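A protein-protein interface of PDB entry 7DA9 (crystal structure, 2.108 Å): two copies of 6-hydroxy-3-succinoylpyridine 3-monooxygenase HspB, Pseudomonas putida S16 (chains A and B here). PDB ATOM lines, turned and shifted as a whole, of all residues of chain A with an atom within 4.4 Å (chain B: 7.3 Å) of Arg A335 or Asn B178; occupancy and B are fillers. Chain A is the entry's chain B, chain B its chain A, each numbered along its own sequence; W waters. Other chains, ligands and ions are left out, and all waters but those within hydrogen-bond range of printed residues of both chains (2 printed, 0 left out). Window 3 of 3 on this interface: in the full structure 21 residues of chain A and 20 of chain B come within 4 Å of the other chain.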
ATOM      1  N   THR A 274      16.130  10.739  27.293  1.00  0.00           N
ATOM      2  CA  THR A 274      17.516  11.047  27.606  1.00  0.00           C
ATOM      3  C   THR A 274      18.398   9.813  27.366  1.00  0.00           C
ATOM      4  O   THR A 274      17.914   8.710  27.094  1.00  0.00           O
ATOM      5  CB  THR A 274      17.638  11.531  29.042  1.00  0.00           C
ATOM      6  OG1 THR A 274      18.974  11.993  29.281  1.00  0.00           O
ATOM      7  CG2 THR A 274      17.308  10.392  30.011  1.00  0.00           C
ATOM      8  N   ASP A 275      19.714  10.012  27.491  1.00  0.00           N
ATOM      9  CA  ASP A 275      20.668   8.949  27.172  1.00  0.00           C
ATOM     10  C   ASP A 275      20.638   7.838  28.216  1.00  0.00           C
ATOM     11  O   ASP A 275      20.778   6.658  27.876  1.00  0.00           O
ATOM     12  CB  ASP A 275      22.088   9.517  27.061  1.00  0.00           C
ATOM     13  CG  ASP A 275      22.140  10.810  26.261  1.00  0.00           C
ATOM     14  OD1 ASP A 275      22.812  10.850  25.203  1.00  0.00           O
ATOM     15  OD2 ASP A 275      21.513  11.797  26.708  1.00  0.00           O
ATOM     16  N   ARG A 276      20.471   8.189  29.488  1.00  0.00           N
ATOM     17  CA  ARG A 276      20.430   7.189  30.543  1.00  0.00           C
ATOM     18  C   ARG A 276      19.624   7.737  31.707  1.00  0.00           C
ATOM     19  O   ARG A 276      19.694   8.929  32.006  1.00  0.00           O
ATOM     20  CB  ARG A 276      21.845   6.820  31.001  1.00  0.00           C
ATOM     21  CG  ARG A 276      22.785   8.005  31.038  1.00  0.00           C
ATOM     22  CD  ARG A 276      24.255   7.597  31.117  1.00  0.00           C
ATOM     23  NE  ARG A 276      25.099   8.515  30.348  1.00  0.00           N
ATOM     24  CZ  ARG A 276      26.285   8.198  29.836  1.00  0.00           C
ATOM     25  NH1 ARG A 276      26.786   6.980  30.009  1.00  0.00           N
ATOM     26  NH2 ARG A 276      26.976   9.098  29.149  1.00  0.00           N
ATOM     27  N   MET A 277      18.863   6.867  32.365  1.00  0.00           N
ATOM     28  CA  MET A 277      18.080   7.272  33.523  1.00  0.00           C
ATOM     29  C   MET A 277      18.797   6.978  34.838  1.00  0.00           C
ATOM     30  O   MET A 277      18.176   7.043  35.904  1.00  0.00           O
ATOM     31  CB  MET A 277      16.703   6.604  33.485  1.00  0.00           C
ATOM     32  CG  MET A 277      15.817   7.112  32.358  1.00  0.00           C
ATOM     33  SD  MET A 277      14.395   6.041  32.130  1.00  0.00           S
ATOM     34  CE  MET A 277      13.453   6.337  33.642  1.00  0.00           C
ATOM     35  N   GLU A 331      17.384   1.207  34.892  1.00  0.00           N
ATOM     36  CA  GLU A 331      17.330   2.339  33.980  1.00  0.00           C
ATOM     37  C   GLU A 331      17.151   1.869  32.544  1.00  0.00           C
ATOM     38  O   GLU A 331      16.346   2.441  31.796  1.00  0.00           O
ATOM     39  CB  GLU A 331      18.571   3.231  34.148  1.00  0.00           C
ATOM     40  CG  GLU A 331      19.849   2.800  33.390  1.00  0.00           C
ATOM     41  CD  GLU A 331      19.838   3.212  31.923  1.00  0.00           C
ATOM     42  OE1 GLU A 331      19.083   4.153  31.565  1.00  0.00           O
ATOM     43  OE2 GLU A 331      20.556   2.571  31.124  1.00  0.00           O
ATOM     44  N   ALA A 332      17.851   0.802  32.158  1.00  0.00           N
ATOM     45  CA  ALA A 332      17.710   0.279  30.802  1.00  0.00           C
ATOM     46  C   ALA A 332      16.303  -0.247  30.553  1.00  0.00           C
ATOM     47  O   ALA A 332      15.741  -0.040  29.466  1.00  0.00           O
ATOM     48  CB  ALA A 332      18.751  -0.810  30.542  1.00  0.00           C
ATOM     49  N   ASP A 333      15.697  -0.918  31.542  1.00  0.00           N
ATOM     50  CA  ASP A 333      14.351  -1.411  31.286  1.00  0.00           C
ATOM     51  C   ASP A 333      13.369  -0.258  31.154  1.00  0.00           C
ATOM     52  O   ASP A 333      12.418  -0.332  30.367  1.00  0.00           O
ATOM     53  CB  ASP A 333      13.871  -2.366  32.370  1.00  0.00           C
ATOM     54  CG  ASP A 333      12.685  -3.194  31.888  1.00  0.00           C
ATOM     55  OD1 ASP A 333      12.823  -3.845  30.819  1.00  0.00           O
ATOM     56  OD2 ASP A 333      11.615  -3.189  32.542  1.00  0.00           O
ATOM     57  N   ARG A 334      13.568   0.812  31.929  1.00  0.00           N
ATOM     58  CA  ARG A 334      12.631   1.928  31.829  1.00  0.00           C
ATOM     59  C   ARG A 334      12.766   2.635  30.488  1.00  0.00           C
ATOM     60  O   ARG A 334      11.762   3.034  29.882  1.00  0.00           O
ATOM     61  CB  ARG A 334      12.836   2.885  32.995  1.00  0.00           C
ATOM     62  CG  ARG A 334      12.351   2.275  34.310  1.00  0.00           C
ATOM     63  CD  ARG A 334      10.871   2.532  34.484  1.00  0.00           C
ATOM     64  NE  ARG A 334      10.044   1.438  34.019  1.00  0.00           N
ATOM     65  CZ  ARG A 334       8.841   1.589  33.476  1.00  0.00           C
ATOM     66  NH1 ARG A 334       8.318   2.801  33.314  1.00  0.00           N
ATOM     67  NH2 ARG A 334       8.158   0.522  33.097  1.00  0.00           N
ATOM     68  N   ARG A 335      13.993   2.764  29.988  1.00  0.00           N
ATOM     69  CA  ARG A 335      14.185   3.293  28.645  1.00  0.00           C
ATOM     70  C   ARG A 335      13.601   2.362  27.586  1.00  0.00           C
ATOM     71  O   ARG A 335      13.000   2.832  26.610  1.00  0.00           O
ATOM     72  CB  ARG A 335      15.671   3.551  28.404  1.00  0.00           C
ATOM     73  CG  ARG A 335      16.179   4.756  29.183  1.00  0.00           C
ATOM     74  CD  ARG A 335      17.473   5.312  28.598  1.00  0.00           C
ATOM     75  NE  ARG A 335      18.589   4.414  28.869  1.00  0.00           N
ATOM     76  CZ  ARG A 335      19.274   3.771  27.931  1.00  0.00           C
ATOM     77  NH1 ARG A 335      18.961   3.933  26.643  1.00  0.00           N
ATOM     78  NH2 ARG A 335      20.268   2.960  28.286  1.00  0.00           N
ATOM     79  N   ARG A 336      13.769   1.040  27.761  1.00  0.00           N
ATOM     80  CA  ARG A 336      13.220   0.070  26.813  1.00  0.00           C
ATOM     81  C   ARG A 336      11.707   0.201  26.711  1.00  0.00           C
ATOM     82  O   ARG A 336      11.151   0.221  25.608  1.00  0.00           O
ATOM     83  CB  ARG A 336      13.598  -1.364  27.218  1.00  0.00           C
ATOM     84  CG  ARG A 336      13.105  -2.438  26.242  1.00  0.00           C
ATOM     85  CD  ARG A 336      13.369  -3.890  26.717  1.00  0.00           C
ATOM     86  NE  ARG A 336      14.482  -3.968  27.662  1.00  0.00           N
ATOM     87  CZ  ARG A 336      15.679  -4.478  27.389  1.00  0.00           C
ATOM     88  NH1 ARG A 336      15.938  -4.974  26.182  1.00  0.00           N
ATOM     89  NH2 ARG A 336      16.620  -4.485  28.331  1.00  0.00           N
ATOM     90  N   LYS A 337      11.021   0.277  27.856  1.00  0.00           N
ATOM     91  CA  LYS A 337       9.571   0.454  27.835  1.00  0.00           C
ATOM     92  C   LYS A 337       9.195   1.712  27.072  1.00  0.00           C
ATOM     93  O   LYS A 337       8.316   1.688  26.205  1.00  0.00           O
ATOM     94  CB  LYS A 337       9.006   0.524  29.256  1.00  0.00           C
ATOM     95  CG  LYS A 337       9.280  -0.707  30.097  1.00  0.00           C
ATOM     96  CD  LYS A 337       8.645  -1.929  29.499  1.00  0.00           C
ATOM     97  CE  LYS A 337       8.614  -3.076  30.513  1.00  0.00           C
ATOM     98  NZ  LYS A 337       8.014  -4.296  29.906  1.00  0.00           N
ATOM     99  N   PHE A 338       9.861   2.825  27.371  1.00  0.00           N
ATOM    100  CA  PHE A 338       9.478   4.068  26.720  1.00  0.00           C
ATOM    101  C   PHE A 338       9.716   4.005  25.221  1.00  0.00           C
ATOM    102  O   PHE A 338       8.829   4.335  24.430  1.00  0.00           O
ATOM    103  CB  PHE A 338      10.222   5.264  27.297  1.00  0.00           C
ATOM    104  CG  PHE A 338       9.815   6.547  26.642  1.00  0.00           C
ATOM    105  CD1 PHE A 338       8.646   7.192  27.033  1.00  0.00           C
ATOM    106  CD2 PHE A 338      10.535   7.057  25.579  1.00  0.00           C
ATOM    107  CE1 PHE A 338       8.243   8.362  26.415  1.00  0.00           C
ATOM    108  CE2 PHE A 338      10.127   8.229  24.944  1.00  0.00           C
ATOM    109  CZ  PHE A 338       8.978   8.876  25.367  1.00  0.00           C
ATOM    110  N   ILE A 339      10.913   3.578  24.813  1.00  0.00           N
ATOM    111  CA  ILE A 339      11.316   3.683  23.414  1.00  0.00           C
ATOM    112  C   ILE A 339      10.586   2.655  22.566  1.00  0.00           C
ATOM    113  O   ILE A 339      10.126   2.955  21.460  1.00  0.00           O
ATOM    114  CB  ILE A 339      12.843   3.524  23.296  1.00  0.00           C
ATOM    115  CG1 ILE A 339      13.558   4.718  23.931  1.00  0.00           C
ATOM    116  CG2 ILE A 339      13.271   3.336  21.830  1.00  0.00           C
ATOM    117  CD1 ILE A 339      14.989   4.412  24.298  1.00  0.00           C
ATOM    118  N   ARG B 171      28.930  -4.159  18.923  1.00  0.00           N
ATOM    119  CA  ARG B 171      27.903  -3.550  19.762  1.00  0.00           C
ATOM    120  C   ARG B 171      27.365  -4.544  20.783  1.00  0.00           C
ATOM    121  O   ARG B 171      27.264  -4.232  21.976  1.00  0.00           O
ATOM    122  CB  ARG B 171      26.754  -3.010  18.910  1.00  0.00           C
ATOM    123  CG  ARG B 171      25.674  -2.352  19.783  1.00  0.00           C
ATOM    124  CD  ARG B 171      24.411  -1.984  18.995  1.00  0.00           C
ATOM    125  NE  ARG B 171      23.648  -3.176  18.682  1.00  0.00           N
ATOM    126  CZ  ARG B 171      23.467  -3.640  17.451  1.00  0.00           C
ATOM    127  NH1 ARG B 171      23.979  -2.992  16.404  1.00  0.00           N
ATOM    128  NH2 ARG B 171      22.769  -4.749  17.267  1.00  0.00           N
ATOM    129  N   ARG B 172      27.004  -5.746  20.332  1.00  0.00           N
ATOM    130  CA  ARG B 172      26.348  -6.710  21.215  1.00  0.00           C
ATOM    131  C   ARG B 172      27.327  -7.344  22.201  1.00  0.00           C
ATOM    132  O   ARG B 172      27.080  -7.341  23.413  1.00  0.00           O
ATOM    133  CB  ARG B 172      25.660  -7.800  20.396  1.00  0.00           C
ATOM    134  CG  ARG B 172      24.695  -7.302  19.341  1.00  0.00           C
ATOM    135  CD  ARG B 172      24.188  -8.465  18.518  1.00  0.00           C
ATOM    136  NE  ARG B 172      25.267  -9.145  17.801  1.00  0.00           N
ATOM    137  CZ  ARG B 172      25.840 -10.278  18.202  1.00  0.00           C
ATOM    138  NH1 ARG B 172      25.442 -10.858  19.323  1.00  0.00           N
ATOM    139  NH2 ARG B 172      26.816 -10.827  17.485  1.00  0.00           N
ATOM    140  N   LEU B 175      30.734  -4.406  23.576  1.00  0.00           N
ATOM    141  CA  LEU B 175      30.206  -3.317  24.392  1.00  0.00           C
ATOM    142  C   LEU B 175      28.972  -3.706  25.193  1.00  0.00           C
ATOM    143  O   LEU B 175      28.653  -3.024  26.173  1.00  0.00           O
ATOM    144  CB  LEU B 175      29.859  -2.102  23.523  1.00  0.00           C
ATOM    145  CG  LEU B 175      31.018  -1.394  22.824  1.00  0.00           C
ATOM    146  CD1 LEU B 175      30.525  -0.162  22.088  1.00  0.00           C
ATOM    147  CD2 LEU B 175      32.090  -1.023  23.828  1.00  0.00           C
ATOM    148  N   ASN B 176      28.268  -4.767  24.799  1.00  0.00           N
ATOM    149  CA  ASN B 176      27.029  -5.167  25.465  1.00  0.00           C
ATOM    150  C   ASN B 176      26.090  -3.965  25.605  1.00  0.00           C
ATOM    151  O   ASN B 176      25.569  -3.666  26.682  1.00  0.00           O
ATOM    152  CB  ASN B 176      27.332  -5.813  26.823  1.00  0.00           C
ATOM    153  CG  ASN B 176      26.172  -6.630  27.364  1.00  0.00           C
ATOM    154  OD1 ASN B 176      25.515  -7.372  26.633  1.00  0.00           O
ATOM    155  ND2 ASN B 176      25.922  -6.502  28.664  1.00  0.00           N
ATOM    156  N   GLN B 177      25.922  -3.237  24.503  1.00  0.00           N
ATOM    157  CA  GLN B 177      25.046  -2.075  24.461  1.00  0.00           C
ATOM    158  C   GLN B 177      23.670  -2.469  23.929  1.00  0.00           C
ATOM    159  O   GLN B 177      23.505  -3.481  23.245  1.00  0.00           O
ATOM    160  CB  GLN B 177      25.654  -0.966  23.596  1.00  0.00           C
ATOM    161  CG  GLN B 177      26.836  -0.215  24.262  1.00  0.00           C
ATOM    162  CD  GLN B 177      27.159   1.116  23.559  1.00  0.00           C
ATOM    163  OE1 GLN B 177      26.495   1.501  22.594  1.00  0.00           O
ATOM    164  NE2 GLN B 177      28.182   1.808  24.040  1.00  0.00           N
ATOM    165  N   ASN B 178      22.679  -1.646  24.253  1.00  0.00           N
ATOM    166  CA  ASN B 178      21.325  -1.880  23.776  1.00  0.00           C
ATOM    167  C   ASN B 178      21.166  -1.375  22.345  1.00  0.00           C
ATOM    168  O   ASN B 178      22.007  -0.639  21.818  1.00  0.00           O
ATOM    169  CB  ASN B 178      20.322  -1.197  24.702  1.00  0.00           C
ATOM    170  CG  ASN B 178      20.483  -1.655  26.136  1.00  0.00           C
ATOM    171  OD1 ASN B 178      20.254  -2.830  26.440  1.00  0.00           O
ATOM    172  ND2 ASN B 178      20.910  -0.746  27.017  1.00  0.00           N
ATOM    173  N   PHE B 179      20.054  -1.771  21.725  1.00  0.00           N
ATOM    174  CA  PHE B 179      19.688  -1.351  20.379  1.00  0.00           C
ATOM    175  C   PHE B 179      18.179  -1.078  20.368  1.00  0.00           C
ATOM    176  O   PHE B 179      17.396  -1.724  19.678  1.00  0.00           O
ATOM    177  CB  PHE B 179      20.108  -2.426  19.372  1.00  0.00           C
ATOM    178  CG  PHE B 179      20.501  -1.888  18.024  1.00  0.00           C
ATOM    179  CD1 PHE B 179      21.296  -0.763  17.909  1.00  0.00           C
ATOM    180  CD2 PHE B 179      20.089  -2.530  16.867  1.00  0.00           C
ATOM    181  CE1 PHE B 179      21.651  -0.271  16.654  1.00  0.00           C
ATOM    182  CE2 PHE B 179      20.455  -2.056  15.626  1.00  0.00           C
ATOM    183  CZ  PHE B 179      21.231  -0.920  15.520  1.00  0.00           C
ATOM    184  N   PHE B 180      17.748  -0.107  21.169  1.00  0.00           N
ATOM    185  CA  PHE B 180      16.322   0.116  21.377  1.00  0.00           C
ATOM    186  C   PHE B 180      15.700   0.830  20.184  1.00  0.00           C
ATOM    187  O   PHE B 180      16.316   1.699  19.561  1.00  0.00           O
ATOM    188  CB  PHE B 180      16.053   0.954  22.641  1.00  0.00           C
ATOM    189  CG  PHE B 180      16.452   0.282  23.932  1.00  0.00           C
ATOM    190  CD1 PHE B 180      16.269  -1.070  24.117  1.00  0.00           C
ATOM    191  CD2 PHE B 180      17.030   1.021  24.960  1.00  0.00           C
ATOM    192  CE1 PHE B 180      16.641  -1.685  25.311  1.00  0.00           C
ATOM    193  CE2 PHE B 180      17.406   0.416  26.153  1.00  0.00           C
ATOM    194  CZ  PHE B 180      17.209  -0.934  26.325  1.00  0.00           C
ATOM    195  N   GLY B 181      14.444   0.506  19.926  1.00  0.00           N
ATOM    196  CA  GLY B 181      13.682   1.103  18.838  1.00  0.00           C
ATOM    197  C   GLY B 181      12.530   0.187  18.468  1.00  0.00           C
ATOM    198  O   GLY B 181      12.004  -0.538  19.316  1.00  0.00           O
ATOM    199  N   VAL B 273      18.663   2.629  17.451  1.00  0.00           N
ATOM    200  CA  VAL B 273      19.930   3.315  17.681  1.00  0.00           C
ATOM    201  C   VAL B 273      20.535   2.809  18.987  1.00  0.00           C
ATOM    202  O   VAL B 273      19.821   2.448  19.928  1.00  0.00           O
ATOM    203  CB  VAL B 273      19.743   4.848  17.695  1.00  0.00           C
ATOM    204  CG1 VAL B 273      18.847   5.299  18.895  1.00  0.00           C
ATOM    205  CG2 VAL B 273      21.116   5.555  17.686  1.00  0.00           C
ATOM    206  N   THR B 274      21.861   2.745  19.029  1.00  0.00           N
ATOM    207  CA  THR B 274      22.533   2.259  20.230  1.00  0.00           C
ATOM    208  C   THR B 274      22.622   3.386  21.268  1.00  0.00           C
ATOM    209  O   THR B 274      22.371   4.558  20.973  1.00  0.00           O
ATOM    210  CB  THR B 274      23.908   1.679  19.857  1.00  0.00           C
ATOM    211  OG1 THR B 274      24.474   0.946  20.952  1.00  0.00           O
ATOM    212  CG2 THR B 274      24.870   2.770  19.415  1.00  0.00           C
ATOM    213  N   ASP B 275      22.965   3.020  22.504  1.00  0.00           N
ATOM    214  CA  ASP B 275      23.007   3.996  23.594  1.00  0.00           C
ATOM    215  C   ASP B 275      24.096   5.046  23.367  1.00  0.00           C
ATOM    216  O   ASP B 275      23.898   6.222  23.672  1.00  0.00           O
ATOM    217  CB  ASP B 275      23.246   3.290  24.939  1.00  0.00           C
ATOM    218  CG  ASP B 275      22.188   2.214  25.253  1.00  0.00           C
ATOM    219  OD1 ASP B 275      20.976   2.440  25.016  1.00  0.00           O
ATOM    220  OD2 ASP B 275      22.576   1.133  25.756  1.00  0.00           O
ATOM    221  N   ARG B 276      25.247   4.642  22.833  1.00  0.00           N
ATOM    222  CA  ARG B 276      26.400   5.518  22.708  1.00  0.00           C
ATOM    223  C   ARG B 276      27.261   5.041  21.547  1.00  0.00           C
ATOM    224  O   ARG B 276      27.509   3.849  21.415  1.00  0.00           O
ATOM    225  CB  ARG B 276      27.222   5.518  24.006  1.00  0.00           C
ATOM    226  CG  ARG B 276      27.808   6.877  24.361  1.00  0.00           C
ATOM    227  CD  ARG B 276      28.529   6.836  25.706  1.00  0.00           C
ATOM    228  NE  ARG B 276      28.657   8.173  26.280  1.00  0.00           N
ATOM    229  CZ  ARG B 276      29.645   9.018  25.998  1.00  0.00           C
ATOM    230  NH1 ARG B 276      30.603   8.664  25.146  1.00  0.00           N
ATOM    231  NH2 ARG B 276      29.677  10.218  26.567  1.00  0.00           N
ATOM    232  N   LEU B 284      31.383   2.973  17.325  1.00  0.00           N
ATOM    233  CA  LEU B 284      30.450   2.314  16.415  1.00  0.00           C
ATOM    234  C   LEU B 284      29.970   3.287  15.334  1.00  0.00           C
ATOM    235  O   LEU B 284      29.599   4.428  15.639  1.00  0.00           O
ATOM    236  CB  LEU B 284      29.245   1.760  17.193  1.00  0.00           C
ATOM    237  CG  LEU B 284      29.576   0.862  18.392  1.00  0.00           C
ATOM    238  CD1 LEU B 284      28.394   0.743  19.343  1.00  0.00           C
ATOM    239  CD2 LEU B 284      29.990  -0.501  17.895  1.00  0.00           C
ATOM    240  N   ALA B 288      25.956  -0.725  12.616  1.00  0.00           N
ATOM    241  CA  ALA B 288      26.300  -1.166  13.964  1.00  0.00           C
ATOM    242  C   ALA B 288      25.838  -0.155  15.007  1.00  0.00           C
ATOM    243  O   ALA B 288      25.579  -0.523  16.159  1.00  0.00           O
ATOM    244  CB  ALA B 288      27.815  -1.386  14.079  1.00  0.00           C
ATOM    245  N   ALA B 289      25.724   1.114  14.617  1.00  0.00           N
ATOM    246  CA  ALA B 289      25.313   2.200  15.495  1.00  0.00           C
ATOM    247  C   ALA B 289      23.827   2.517  15.418  1.00  0.00           C
ATOM    248  O   ALA B 289      23.236   2.916  16.424  1.00  0.00           O
ATOM    249  CB  ALA B 289      26.110   3.472  15.156  1.00  0.00           C
HETATM  250  O   HOH W   1      18.749  -4.543  25.219  1.00  0.00           O
HETATM  251  O   HOH W   2      20.913   6.591  24.592  1.00  0.00           O
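OD1 of Asp B275 is in salt-bridge range of NH1 of Arg A335 (3.0 Å).
The guanidinium group (NE) of Arg B276 sits close to the guanidinium group (NH2) of Arg A276, 3.5 Å away.
The backbone carbonyl oxygen (O) of Arg B276 lies close to the side-chain amide oxygen (OE1) of Gln B177 (2.8 Å).
O of Asn B178 is in hydrogen-bond range of OG1 of Thr B274, at 3.1 Å.
The backbone carbonyl oxygen (O) of Phe B180 is in hydrogen-bond range of the backbone NH (N) of Val B273, at 3.3 Å.
The guanidinium group (NE) of Arg A335 lies close to the backbone carbonyl oxygen (O) of Asp A275 (3.3 Å).
The side-chain carboxylate (OE1) of Glu A331 is in salt-bridge range of the guanidinium group (NE) of Arg A335, at 2.8 Å.
The guanidinium group (NE) of Arg A336 is in salt-bridge range of the side-chain carboxylate (OD1) of Asp A333 (3.6 Å).
Among the printed residues, merely in contact across the chains: Arg A336 with Phe B180 (3.5 Å), Ala A332 with Phe B180 (3.6 Å), Ile A339 with Gly B181 (3.6 Å), Ile A339 with Phe B180 (3.8 Å), Arg A335 with Phe B180 (3.9 Å) and Arg A335 with Asn B178 (3.97 Å).
Arg A335 touches three residues of chain B.
Asn B178 touches one residue of chain A.
Of the printed residues of chain A, Phe B180 touches Ala A332 (3.6 Å), Arg A335 (3.9 Å), Arg A336 (3.5 Å) and Ile A339 (3.8 Å).
Of the printed residues of chain B, Ala A332 touches Phe B180 (3.6 Å).
Of the printed residues of chain A, Arg B276 touches Arg A276.
Arg A334 touches none of the printed residues of chain B.
Of the 13 printed residues of chain A, 5 touch a printed residue of chain B.
Hydrophobic or aromatic side chains of chain B that line the printed part of chain A: Phe B180.
Among the printed residues, 8 pairs touch across the chains.
Among the printed residues, Asp or Glu carboxylates within 4 Å of a Lys or Arg side-chain nitrogen of the other chain: Arg A335 with Asp B275.
Arg B276 touches its own counterpart, Arg A276.
Positions printed for both chains: 274, 275 and 276.
Of the 8 pairs that touch across the chains among the printed residues, 1 has its exchanged pair printed and touching as well.
Water W1 lies within hydrogen-bond range of OD1 of Asn B178 (2.6 Å) and NH1 of Arg A336 (3.0 Å).
Water W2 bridges the backbone carbonyl oxygen of Asp B275 (3.1 Å) and the backbone carbonyl oxygen of Asp A275 (3.3 Å).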
